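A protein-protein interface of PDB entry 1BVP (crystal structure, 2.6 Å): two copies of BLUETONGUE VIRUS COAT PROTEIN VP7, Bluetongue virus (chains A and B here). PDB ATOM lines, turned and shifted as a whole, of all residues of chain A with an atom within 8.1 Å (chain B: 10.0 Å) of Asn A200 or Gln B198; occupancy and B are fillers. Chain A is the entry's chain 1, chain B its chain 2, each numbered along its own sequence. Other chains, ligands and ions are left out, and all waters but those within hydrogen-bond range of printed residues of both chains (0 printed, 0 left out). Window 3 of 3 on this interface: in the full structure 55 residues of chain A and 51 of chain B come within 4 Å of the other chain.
O of Met A196 is in hydrogen-bond range of NH1 of Arg A140, 3.4 Å away. The guanidinium group of Arg A140 sits at hydrogen-bond distance from the backbone carbonyl oxygen of Ala A197 (3.3 Å). The backbone NH (N) of Trp A141 lies within hydrogen-bond range of the backbone carbonyl oxygen (O) of Ala A195, at 2.8 Å. The side-chain amide oxygen (OE1) of Gln A203 sits at hydrogen-bond distance from the side-chain amide nitrogen (ND2) of Asn A193 (3.0 Å). The guanidinium group of Arg B140 is in hydrogen-bond range of the backbone carbonyl oxygen of Ala B197 (3.3 Å). N of Trp B141 is in hydrogen-bond range of O of Ala B195 (2.8 Å).
Among the printed residues, merely in contact across the chains: Ala A195 with Arg B140 (3.4 Å), Asn A200 with Ala B197 (3.4 Å), Asn A193 with Phe B142 (3.5 Å), Asn A193 with Arg B140 (3.6 Å), Asn A200 with Gln B198 (3.7 Å), Asn A193 with Trp B141 (3.7 Å), Ala A195 with Gln B137 (3.8 Å), Gly A199 with Ala B197 (3.8 Å), Asn A200 with Arg B140 (3.8 Å), Arg A140 with Gln B137 (3.96 Å) and Gln A203 with Phe B142 (3.99 Å).
Hydrophobic or aromatic side chains of chain A that line the printed part of chain B: Ala A195. Of the 13 printed residues of chain B, 7 touch a printed residue of chain A. Hydrophobic or aromatic side chains of chain B within 4 Å of the printed part of chain A: Phe B142. Along chain B the printed residues that touch a printed residue of chain A span positions 137 to 199. Among the printed residues, 18 pairs touch across the chains. Among the printed residues, no Asp or Glu carboxylate lies within 4 Å of a Lys or Arg side-chain nitrogen of the other chain.
The side-chain amide nitrogen (NE2) of Gln B137 is in hydrogen-bond range of the backbone carbonyl oxygen (O) of Gly A139, at 3.3 Å. O of Asn A193 lies within hydrogen-bond range of N of Gln B137, 3.0 Å away. The backbone carbonyl oxygen (O) of Gly A199 lies within hydrogen-bond range of the guanidinium group (NH2) of Arg B140. The backbone carbonyl oxygen (O) of Gly A199 lies close to the backbone NH (N) of Gly B199 (3.4 Å). The side-chain hydroxyl of Ser A201 lies within hydrogen-bond range of the guanidinium group of Arg B140, 2.9 Å away. The backbone NH (N) of Ser A201 sits at hydrogen-bond distance from the backbone carbonyl oxygen (O) of Ala B197, 3.1 Å away. O of Gly A199 lies close to O of Gln B198 (3.2 Å).
Ala A195 touches Arg B140, but with the chains exchanged Arg A140 does not touch Ala B195 (6.3 Å). Gly A199 touches Arg B140, but with the chains exchanged Arg A140 does not touch Gly B199 (5.7 Å). Gly A199 touches Ala B197, but with the chains exchanged Ala A197 does not touch Gly B199 (8.3 Å). Ser A201 touches Ala B197, but with the chains exchanged Ala A197 does not touch Ser B201 (12.2 Å). Positions printed for both chains: 140, 141, 194, 195, 196, 197, 198, 199, 200, 201 and 202. Of the 18 pairs that touch across the chains among the printed residues, 1 has its exchanged pair printed and touching as well.
No residue of chain B comes within 4 Å of Met A196. Printed residues of chain B within 4 Å of Asn A200: Arg B140 (3.8 Å), Ala B197 (3.4 Å) and Gln B198 (3.7 Å). Of the printed residues of chain A, Gln B137 touches Gly A139, Arg A140, Asn A193 and Ala A195. Ala B195 touches none of the printed residues of chain A. Met B196 touches none of the printed residues of chain A. Of chain A, only Gly A199 (3.8 Å), Asn A200 (3.4 Å) and Ser A201 (3.1 Å) come within 4 Å of Ala B197. Gln B198 touches two residues of chain A. Of the printed residues of chain A, Gly B199 touches Gly A199 (3.0 Å).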
ATOM      1  N   GLY A 139     -13.442  10.085  19.854  1.00  0.00           N
ATOM      2  CA  GLY A 139     -12.267   9.240  19.899  1.00  0.00           C
ATOM      3  C   GLY A 139     -10.936   9.905  20.164  1.00  0.00           C
ATOM      4  O   GLY A 139      -9.908   9.361  19.776  1.00  0.00           O
ATOM      5  N   ARG A 140     -10.962  11.115  20.719  1.00  0.00           N
ATOM      6  CA  ARG A 140      -9.750  11.825  21.067  1.00  0.00           C
ATOM      7  C   ARG A 140      -9.811  12.013  22.568  1.00  0.00           C
ATOM      8  O   ARG A 140     -10.835  12.410  23.127  1.00  0.00           O
ATOM      9  CB  ARG A 140      -9.603  13.167  20.348  1.00  0.00           C
ATOM     10  CG  ARG A 140      -8.656  14.121  21.075  1.00  0.00           C
ATOM     11  CD  ARG A 140      -8.314  15.334  20.253  1.00  0.00           C
ATOM     12  NE  ARG A 140      -7.671  14.921  19.013  1.00  0.00           N
ATOM     13  CZ  ARG A 140      -6.363  14.943  18.767  1.00  0.00           C
ATOM     14  NH1 ARG A 140      -5.501  15.385  19.676  1.00  0.00           N
ATOM     15  NH2 ARG A 140      -5.921  14.435  17.627  1.00  0.00           N
ATOM     16  N   TRP A 141      -8.714  11.626  23.199  1.00  0.00           N
ATOM     17  CA  TRP A 141      -8.521  11.680  24.628  1.00  0.00           C
ATOM     18  C   TRP A 141      -8.716  13.075  25.188  1.00  0.00           C
ATOM     19  O   TRP A 141      -8.377  14.092  24.563  1.00  0.00           O
ATOM     20  CB  TRP A 141      -7.106  11.186  24.925  1.00  0.00           C
ATOM     21  CG  TRP A 141      -6.721  11.262  26.360  1.00  0.00           C
ATOM     22  CD1 TRP A 141      -6.183  12.349  27.023  1.00  0.00           C
ATOM     23  CD2 TRP A 141      -6.864  10.223  27.341  1.00  0.00           C
ATOM     24  NE1 TRP A 141      -5.995  12.040  28.354  1.00  0.00           N
ATOM     25  CE2 TRP A 141      -6.396  10.747  28.578  1.00  0.00           C
ATOM     26  CE3 TRP A 141      -7.347   8.903  27.296  1.00  0.00           C
ATOM     27  CZ2 TRP A 141      -6.397   9.996  29.757  1.00  0.00           C
ATOM     28  CZ3 TRP A 141      -7.352   8.154  28.466  1.00  0.00           C
ATOM     29  CH2 TRP A 141      -6.875   8.710  29.687  1.00  0.00           C
ATOM     30  N   ASN A 193      -9.168   2.180  19.106  1.00  0.00           N
ATOM     31  CA  ASN A 193      -8.056   2.985  18.591  1.00  0.00           C
ATOM     32  C   ASN A 193      -8.448   4.430  18.737  1.00  0.00           C
ATOM     33  O   ASN A 193      -9.396   4.857  18.086  1.00  0.00           O
ATOM     34  CB  ASN A 193      -7.852   2.686  17.102  1.00  0.00           C
ATOM     35  CG  ASN A 193      -6.512   3.179  16.564  1.00  0.00           C
ATOM     36  OD1 ASN A 193      -6.446   3.844  15.525  1.00  0.00           O
ATOM     37  ND2 ASN A 193      -5.437   2.762  17.204  1.00  0.00           N
ATOM     38  N   PHE A 194      -7.780   5.158  19.627  1.00  0.00           N
ATOM     39  CA  PHE A 194      -8.085   6.573  19.846  1.00  0.00           C
ATOM     40  C   PHE A 194      -6.849   7.479  19.772  1.00  0.00           C
ATOM     41  O   PHE A 194      -5.727   7.017  19.775  1.00  0.00           O
ATOM     42  CB  PHE A 194      -8.790   6.778  21.187  1.00  0.00           C
ATOM     43  CG  PHE A 194      -7.998   6.304  22.382  1.00  0.00           C
ATOM     44  CD1 PHE A 194      -7.965   4.952  22.721  1.00  0.00           C
ATOM     45  CD2 PHE A 194      -7.366   7.223  23.226  1.00  0.00           C
ATOM     46  CE1 PHE A 194      -7.323   4.516  23.895  1.00  0.00           C
ATOM     47  CE2 PHE A 194      -6.723   6.803  24.403  1.00  0.00           C
ATOM     48  CZ  PHE A 194      -6.704   5.454  24.740  1.00  0.00           C
ATOM     49  N   ALA A 195      -7.077   8.778  19.714  1.00  0.00           N
ATOM     50  CA  ALA A 195      -6.025   9.757  19.620  1.00  0.00           C
ATOM     51  C   ALA A 195      -5.671  10.281  20.983  1.00  0.00           C
ATOM     52  O   ALA A 195      -6.566  10.625  21.766  1.00  0.00           O
ATOM     53  CB  ALA A 195      -6.462  10.915  18.741  1.00  0.00           C
ATOM     54  N   MET A 196      -4.365  10.346  21.263  1.00  0.00           N
ATOM     55  CA  MET A 196      -3.874  10.884  22.529  1.00  0.00           C
ATOM     56  C   MET A 196      -3.823  12.400  22.334  1.00  0.00           C
ATOM     57  O   MET A 196      -3.880  12.870  21.192  1.00  0.00           O
ATOM     58  CB  MET A 196      -2.528  10.277  22.848  1.00  0.00           C
ATOM     59  CG  MET A 196      -2.625   8.873  23.420  1.00  0.00           C
ATOM     60  SD  MET A 196      -3.326   8.851  25.139  1.00  0.00           S
ATOM     61  CE  MET A 196      -3.144  10.702  25.718  1.00  0.00           C
ATOM     62  N   ALA A 197      -3.734  13.184  23.407  1.00  0.00           N
ATOM     63  CA  ALA A 197      -3.731  14.653  23.248  1.00  0.00           C
ATOM     64  C   ALA A 197      -2.719  15.164  22.210  1.00  0.00           C
ATOM     65  O   ALA A 197      -2.931  16.172  21.516  1.00  0.00           O
ATOM     66  CB  ALA A 197      -3.514  15.324  24.588  1.00  0.00           C
ATOM     67  N   GLN A 198      -1.604  14.457  22.130  1.00  0.00           N
ATOM     68  CA  GLN A 198      -0.551  14.779  21.198  1.00  0.00           C
ATOM     69  C   GLN A 198      -0.891  14.401  19.771  1.00  0.00           C
ATOM     70  O   GLN A 198      -0.393  14.994  18.848  1.00  0.00           O
ATOM     71  CB  GLN A 198       0.777  14.166  21.662  1.00  0.00           C
ATOM     72  CG  GLN A 198       1.570  15.131  22.531  1.00  0.00           C
ATOM     73  CD  GLN A 198       1.589  16.580  21.936  1.00  0.00           C
ATOM     74  OE1 GLN A 198       1.929  16.790  20.755  1.00  0.00           O
ATOM     75  NE2 GLN A 198       1.189  17.564  22.747  1.00  0.00           N
ATOM     76  N   GLY A 199      -1.716  13.393  19.562  1.00  0.00           N
ATOM     77  CA  GLY A 199      -2.055  13.070  18.196  1.00  0.00           C
ATOM     78  C   GLY A 199      -1.753  11.653  17.834  1.00  0.00           C
ATOM     79  O   GLY A 199      -2.243  11.162  16.825  1.00  0.00           O
ATOM     80  N   ASN A 200      -1.030  10.959  18.695  1.00  0.00           N
ATOM     81  CA  ASN A 200      -0.645   9.584  18.398  1.00  0.00           C
ATOM     82  C   ASN A 200      -1.720   8.592  18.847  1.00  0.00           C
ATOM     83  O   ASN A 200      -2.416   8.819  19.855  1.00  0.00           O
ATOM     84  CB  ASN A 200       0.711   9.267  19.067  1.00  0.00           C
ATOM     85  CG  ASN A 200       0.659   9.427  20.580  1.00  0.00           C
ATOM     86  OD1 ASN A 200       0.762   8.436  21.316  1.00  0.00           O
ATOM     87  ND2 ASN A 200       0.448  10.674  21.059  1.00  0.00           N
ATOM     88  N   SER A 201      -1.847   7.498  18.103  1.00  0.00           N
ATOM     89  CA  SER A 201      -2.815   6.467  18.419  1.00  0.00           C
ATOM     90  C   SER A 201      -2.497   5.704  19.691  1.00  0.00           C
ATOM     91  O   SER A 201      -1.353   5.506  20.042  1.00  0.00           O
ATOM     92  CB  SER A 201      -2.900   5.480  17.269  1.00  0.00           C
ATOM     93  OG  SER A 201      -3.245   6.159  16.073  1.00  0.00           O
ATOM     94  N   GLN A 202      -3.537   5.201  20.330  1.00  0.00           N
ATOM     95  CA  GLN A 202      -3.412   4.422  21.545  1.00  0.00           C
ATOM     96  C   GLN A 202      -4.551   3.373  21.487  1.00  0.00           C
ATOM     97  O   GLN A 202      -5.567   3.582  20.822  1.00  0.00           O
ATOM     98  CB  GLN A 202      -3.542   5.350  22.750  1.00  0.00           C
ATOM     99  CG  GLN A 202      -3.399   4.665  24.084  1.00  0.00           C
ATOM    100  CD  GLN A 202      -1.969   4.580  24.553  1.00  0.00           C
ATOM    101  OE1 GLN A 202      -1.071   5.182  23.956  1.00  0.00           O
ATOM    102  NE2 GLN A 202      -1.744   3.834  25.629  1.00  0.00           N
ATOM    103  N   GLN A 203      -4.346   2.223  22.118  1.00  0.00           N
ATOM    104  CA  GLN A 203      -5.341   1.151  22.132  1.00  0.00           C
ATOM    105  C   GLN A 203      -5.970   1.020  23.501  1.00  0.00           C
ATOM    106  O   GLN A 203      -5.354   1.372  24.516  1.00  0.00           O
ATOM    107  CB  GLN A 203      -4.678  -0.191  21.873  1.00  0.00           C
ATOM    108  CG  GLN A 203      -5.110  -0.872  20.633  1.00  0.00           C
ATOM    109  CD  GLN A 203      -4.329  -0.392  19.452  1.00  0.00           C
ATOM    110  OE1 GLN A 203      -4.224   0.819  19.197  1.00  0.00           O
ATOM    111  NE2 GLN A 203      -3.717  -1.337  18.739  1.00  0.00           N
ATOM    112  N   GLN B 137     -11.765   5.134  16.348  1.00  0.00           N
ATOM    113  CA  GLN B 137     -11.955   6.564  16.070  1.00  0.00           C
ATOM    114  C   GLN B 137     -12.168   6.818  14.589  1.00  0.00           C
ATOM    115  O   GLN B 137     -11.385   6.370  13.724  1.00  0.00           O
ATOM    116  CB  GLN B 137     -10.790   7.415  16.516  1.00  0.00           C
ATOM    117  CG  GLN B 137     -11.027   8.886  16.220  1.00  0.00           C
ATOM    118  CD  GLN B 137      -9.801   9.755  16.415  1.00  0.00           C
ATOM    119  OE1 GLN B 137      -8.700   9.338  16.125  1.00  0.00           O
ATOM    120  NE2 GLN B 137     -10.001  10.975  16.876  1.00  0.00           N
ATOM    121  N   ARG B 140      -9.298   7.994  11.443  1.00  0.00           N
ATOM    122  CA  ARG B 140      -7.927   7.837  11.876  1.00  0.00           C
ATOM    123  C   ARG B 140      -7.479   6.502  11.318  1.00  0.00           C
ATOM    124  O   ARG B 140      -8.183   5.494  11.414  1.00  0.00           O
ATOM    125  CB  ARG B 140      -7.757   7.883  13.396  1.00  0.00           C
ATOM    126  CG  ARG B 140      -6.468   7.211  13.863  1.00  0.00           C
ATOM    127  CD  ARG B 140      -6.174   7.471  15.316  1.00  0.00           C
ATOM    128  NE  ARG B 140      -6.041   8.904  15.541  1.00  0.00           N
ATOM    129  CZ  ARG B 140      -4.896   9.573  15.656  1.00  0.00           C
ATOM    130  NH1 ARG B 140      -3.726   8.947  15.589  1.00  0.00           N
ATOM    131  NH2 ARG B 140      -4.936  10.892  15.752  1.00  0.00           N
ATOM    132  N   TRP B 141      -6.335   6.556  10.656  1.00  0.00           N
ATOM    133  CA  TRP B 141      -5.699   5.433  10.010  1.00  0.00           C
ATOM    134  C   TRP B 141      -5.441   4.285  10.966  1.00  0.00           C
ATOM    135  O   TRP B 141      -5.126   4.469  12.152  1.00  0.00           O
ATOM    136  CB  TRP B 141      -4.385   5.925   9.409  1.00  0.00           C
ATOM    137  CG  TRP B 141      -3.565   4.857   8.777  1.00  0.00           C
ATOM    138  CD1 TRP B 141      -2.649   4.029   9.400  1.00  0.00           C
ATOM    139  CD2 TRP B 141      -3.590   4.462   7.396  1.00  0.00           C
ATOM    140  NE1 TRP B 141      -2.119   3.144   8.484  1.00  0.00           N
ATOM    141  CE2 TRP B 141      -2.669   3.387   7.250  1.00  0.00           C
ATOM    142  CE3 TRP B 141      -4.305   4.908   6.271  1.00  0.00           C
ATOM    143  CZ2 TRP B 141      -2.445   2.755   6.025  1.00  0.00           C
ATOM    144  CZ3 TRP B 141      -4.087   4.279   5.050  1.00  0.00           C
ATOM    145  CH2 TRP B 141      -3.157   3.208   4.941  1.00  0.00           C
ATOM    146  N   PHE B 142      -5.608   3.080  10.453  1.00  0.00           N
ATOM    147  CA  PHE B 142      -5.349   1.888  11.255  1.00  0.00           C
ATOM    148  C   PHE B 142      -5.247   0.688  10.348  1.00  0.00           C
ATOM    149  O   PHE B 142      -6.176   0.361   9.590  1.00  0.00           O
ATOM    150  CB  PHE B 142      -6.390   1.674  12.331  1.00  0.00           C
ATOM    151  CG  PHE B 142      -6.166   0.446  13.138  1.00  0.00           C
ATOM    152  CD1 PHE B 142      -6.521  -0.803  12.638  1.00  0.00           C
ATOM    153  CD2 PHE B 142      -5.580   0.531  14.404  1.00  0.00           C
ATOM    154  CE1 PHE B 142      -6.291  -1.969  13.391  1.00  0.00           C
ATOM    155  CE2 PHE B 142      -5.341  -0.620  15.164  1.00  0.00           C
ATOM    156  CZ  PHE B 142      -5.695  -1.876  14.660  1.00  0.00           C
ATOM    157  N   PHE B 194      -7.811  12.689   6.695  1.00  0.00           N
ATOM    158  CA  PHE B 194      -7.757  11.771   7.834  1.00  0.00           C
ATOM    159  C   PHE B 194      -6.457  11.881   8.642  1.00  0.00           C
ATOM    160  O   PHE B 194      -5.500  12.492   8.216  1.00  0.00           O
ATOM    161  CB  PHE B 194      -7.956  10.325   7.380  1.00  0.00           C
ATOM    162  CG  PHE B 194      -6.938   9.846   6.374  1.00  0.00           C
ATOM    163  CD1 PHE B 194      -7.058  10.180   5.027  1.00  0.00           C
ATOM    164  CD2 PHE B 194      -5.911   8.977   6.761  1.00  0.00           C
ATOM    165  CE1 PHE B 194      -6.178   9.646   4.067  1.00  0.00           C
ATOM    166  CE2 PHE B 194      -5.026   8.435   5.815  1.00  0.00           C
ATOM    167  CZ  PHE B 194      -5.159   8.764   4.470  1.00  0.00           C
ATOM    168  N   ALA B 195      -6.440  11.270   9.812  1.00  0.00           N
ATOM    169  CA  ALA B 195      -5.303  11.297  10.695  1.00  0.00           C
ATOM    170  C   ALA B 195      -4.449  10.077  10.491  1.00  0.00           C
ATOM    171  O   ALA B 195      -4.973   8.957  10.431  1.00  0.00           O
ATOM    172  CB  ALA B 195      -5.764  11.344  12.141  1.00  0.00           C
ATOM    173  N   MET B 196      -3.134  10.296  10.390  1.00  0.00           N
ATOM    174  CA  MET B 196      -2.179   9.199  10.242  1.00  0.00           C
ATOM    175  C   MET B 196      -1.904   8.706  11.663  1.00  0.00           C
ATOM    176  O   MET B 196      -2.223   9.411  12.627  1.00  0.00           O
ATOM    177  CB  MET B 196      -0.943   9.698   9.532  1.00  0.00           C
ATOM    178  CG  MET B 196      -1.122   9.816   8.028  1.00  0.00           C
ATOM    179  SD  MET B 196      -1.244   8.163   7.193  1.00  0.00           S
ATOM    180  CE  MET B 196      -0.541   6.936   8.531  1.00  0.00           C
ATOM    181  N   ALA B 197      -1.337   7.512  11.831  1.00  0.00           N
ATOM    182  CA  ALA B 197      -1.105   6.992  13.194  1.00  0.00           C
ATOM    183  C   ALA B 197      -0.389   7.986  14.124  1.00  0.00           C
ATOM    184  O   ALA B 197      -0.611   8.029  15.345  1.00  0.00           O
ATOM    185  CB  ALA B 197      -0.357   5.678  13.131  1.00  0.00           C
ATOM    186  N   GLN B 198       0.490   8.770  13.524  1.00  0.00           N
ATOM    187  CA  GLN B 198       1.241   9.775  14.236  1.00  0.00           C
ATOM    188  C   GLN B 198       0.408  10.987  14.599  1.00  0.00           C
ATOM    189  O   GLN B 198       0.697  11.661  15.555  1.00  0.00           O
ATOM    190  CB  GLN B 198       2.505  10.152  13.452  1.00  0.00           C
ATOM    191  CG  GLN B 198       3.698   9.301  13.863  1.00  0.00           C
ATOM    192  CD  GLN B 198       3.806   9.153  15.420  1.00  0.00           C
ATOM    193  OE1 GLN B 198       3.795  10.151  16.167  1.00  0.00           O
ATOM    194  NE2 GLN B 198       3.874   7.907  15.897  1.00  0.00           N
ATOM    195  N   GLY B 199      -0.618  11.304  13.831  1.00  0.00           N
ATOM    196  CA  GLY B 199      -1.420  12.443  14.213  1.00  0.00           C
ATOM    197  C   GLY B 199      -1.521  13.476  13.142  1.00  0.00           C
ATOM    198  O   GLY B 199      -2.386  14.342  13.206  1.00  0.00           O
ATOM    199  N   ASN B 200      -0.712  13.343  12.105  1.00  0.00           N
ATOM    200  CA  ASN B 200      -0.709  14.336  11.037  1.00  0.00           C
ATOM    201  C   ASN B 200      -1.759  14.016   9.971  1.00  0.00           C
ATOM    202  O   ASN B 200      -2.049  12.836   9.697  1.00  0.00           O
ATOM    203  CB  ASN B 200       0.701  14.424  10.413  1.00  0.00           C
ATOM    204  CG  ASN B 200       1.156  13.094   9.824  1.00  0.00           C
ATOM    205  OD1 ASN B 200       1.293  12.969   8.599  1.00  0.00           O
ATOM    206  ND2 ASN B 200       1.345  12.073  10.690  1.00  0.00           N
ATOM    207  N   SER B 201      -2.317  15.064   9.374  1.00  0.00           N
ATOM    208  CA  SER B 201      -3.316  14.909   8.336  1.00  0.00           C
ATOM    209  C   SER B 201      -2.769  14.322   7.049  1.00  0.00           C
ATOM    210  O   SER B 201      -1.633  14.540   6.685  1.00  0.00           O
ATOM    211  CB  SER B 201      -3.942  16.257   8.027  1.00  0.00           C
ATOM    212  OG  SER B 201      -4.506  16.810   9.204  1.00  0.00           O
ATOM    213  N   GLN B 202      -3.634  13.642   6.318  1.00  0.00           N
ATOM    214  CA  GLN B 202      -3.287  13.038   5.048  1.00  0.00           C
ATOM    215  C   GLN B 202      -4.566  13.135   4.177  1.00  0.00           C
ATOM    216  O   GLN B 202      -5.679  13.217   4.699  1.00  0.00           O
ATOM    217  CB  GLN B 202      -2.856  11.593   5.282  1.00  0.00           C
ATOM    218  CG  GLN B 202      -2.438  10.857   4.036  1.00  0.00           C
ATOM    219  CD  GLN B 202      -0.977  11.031   3.711  1.00  0.00           C
ATOM    220  OE1 GLN B 202      -0.212  11.581   4.509  1.00  0.00           O
ATOM    221  NE2 GLN B 202      -0.574  10.563   2.534  1.00  0.00           N
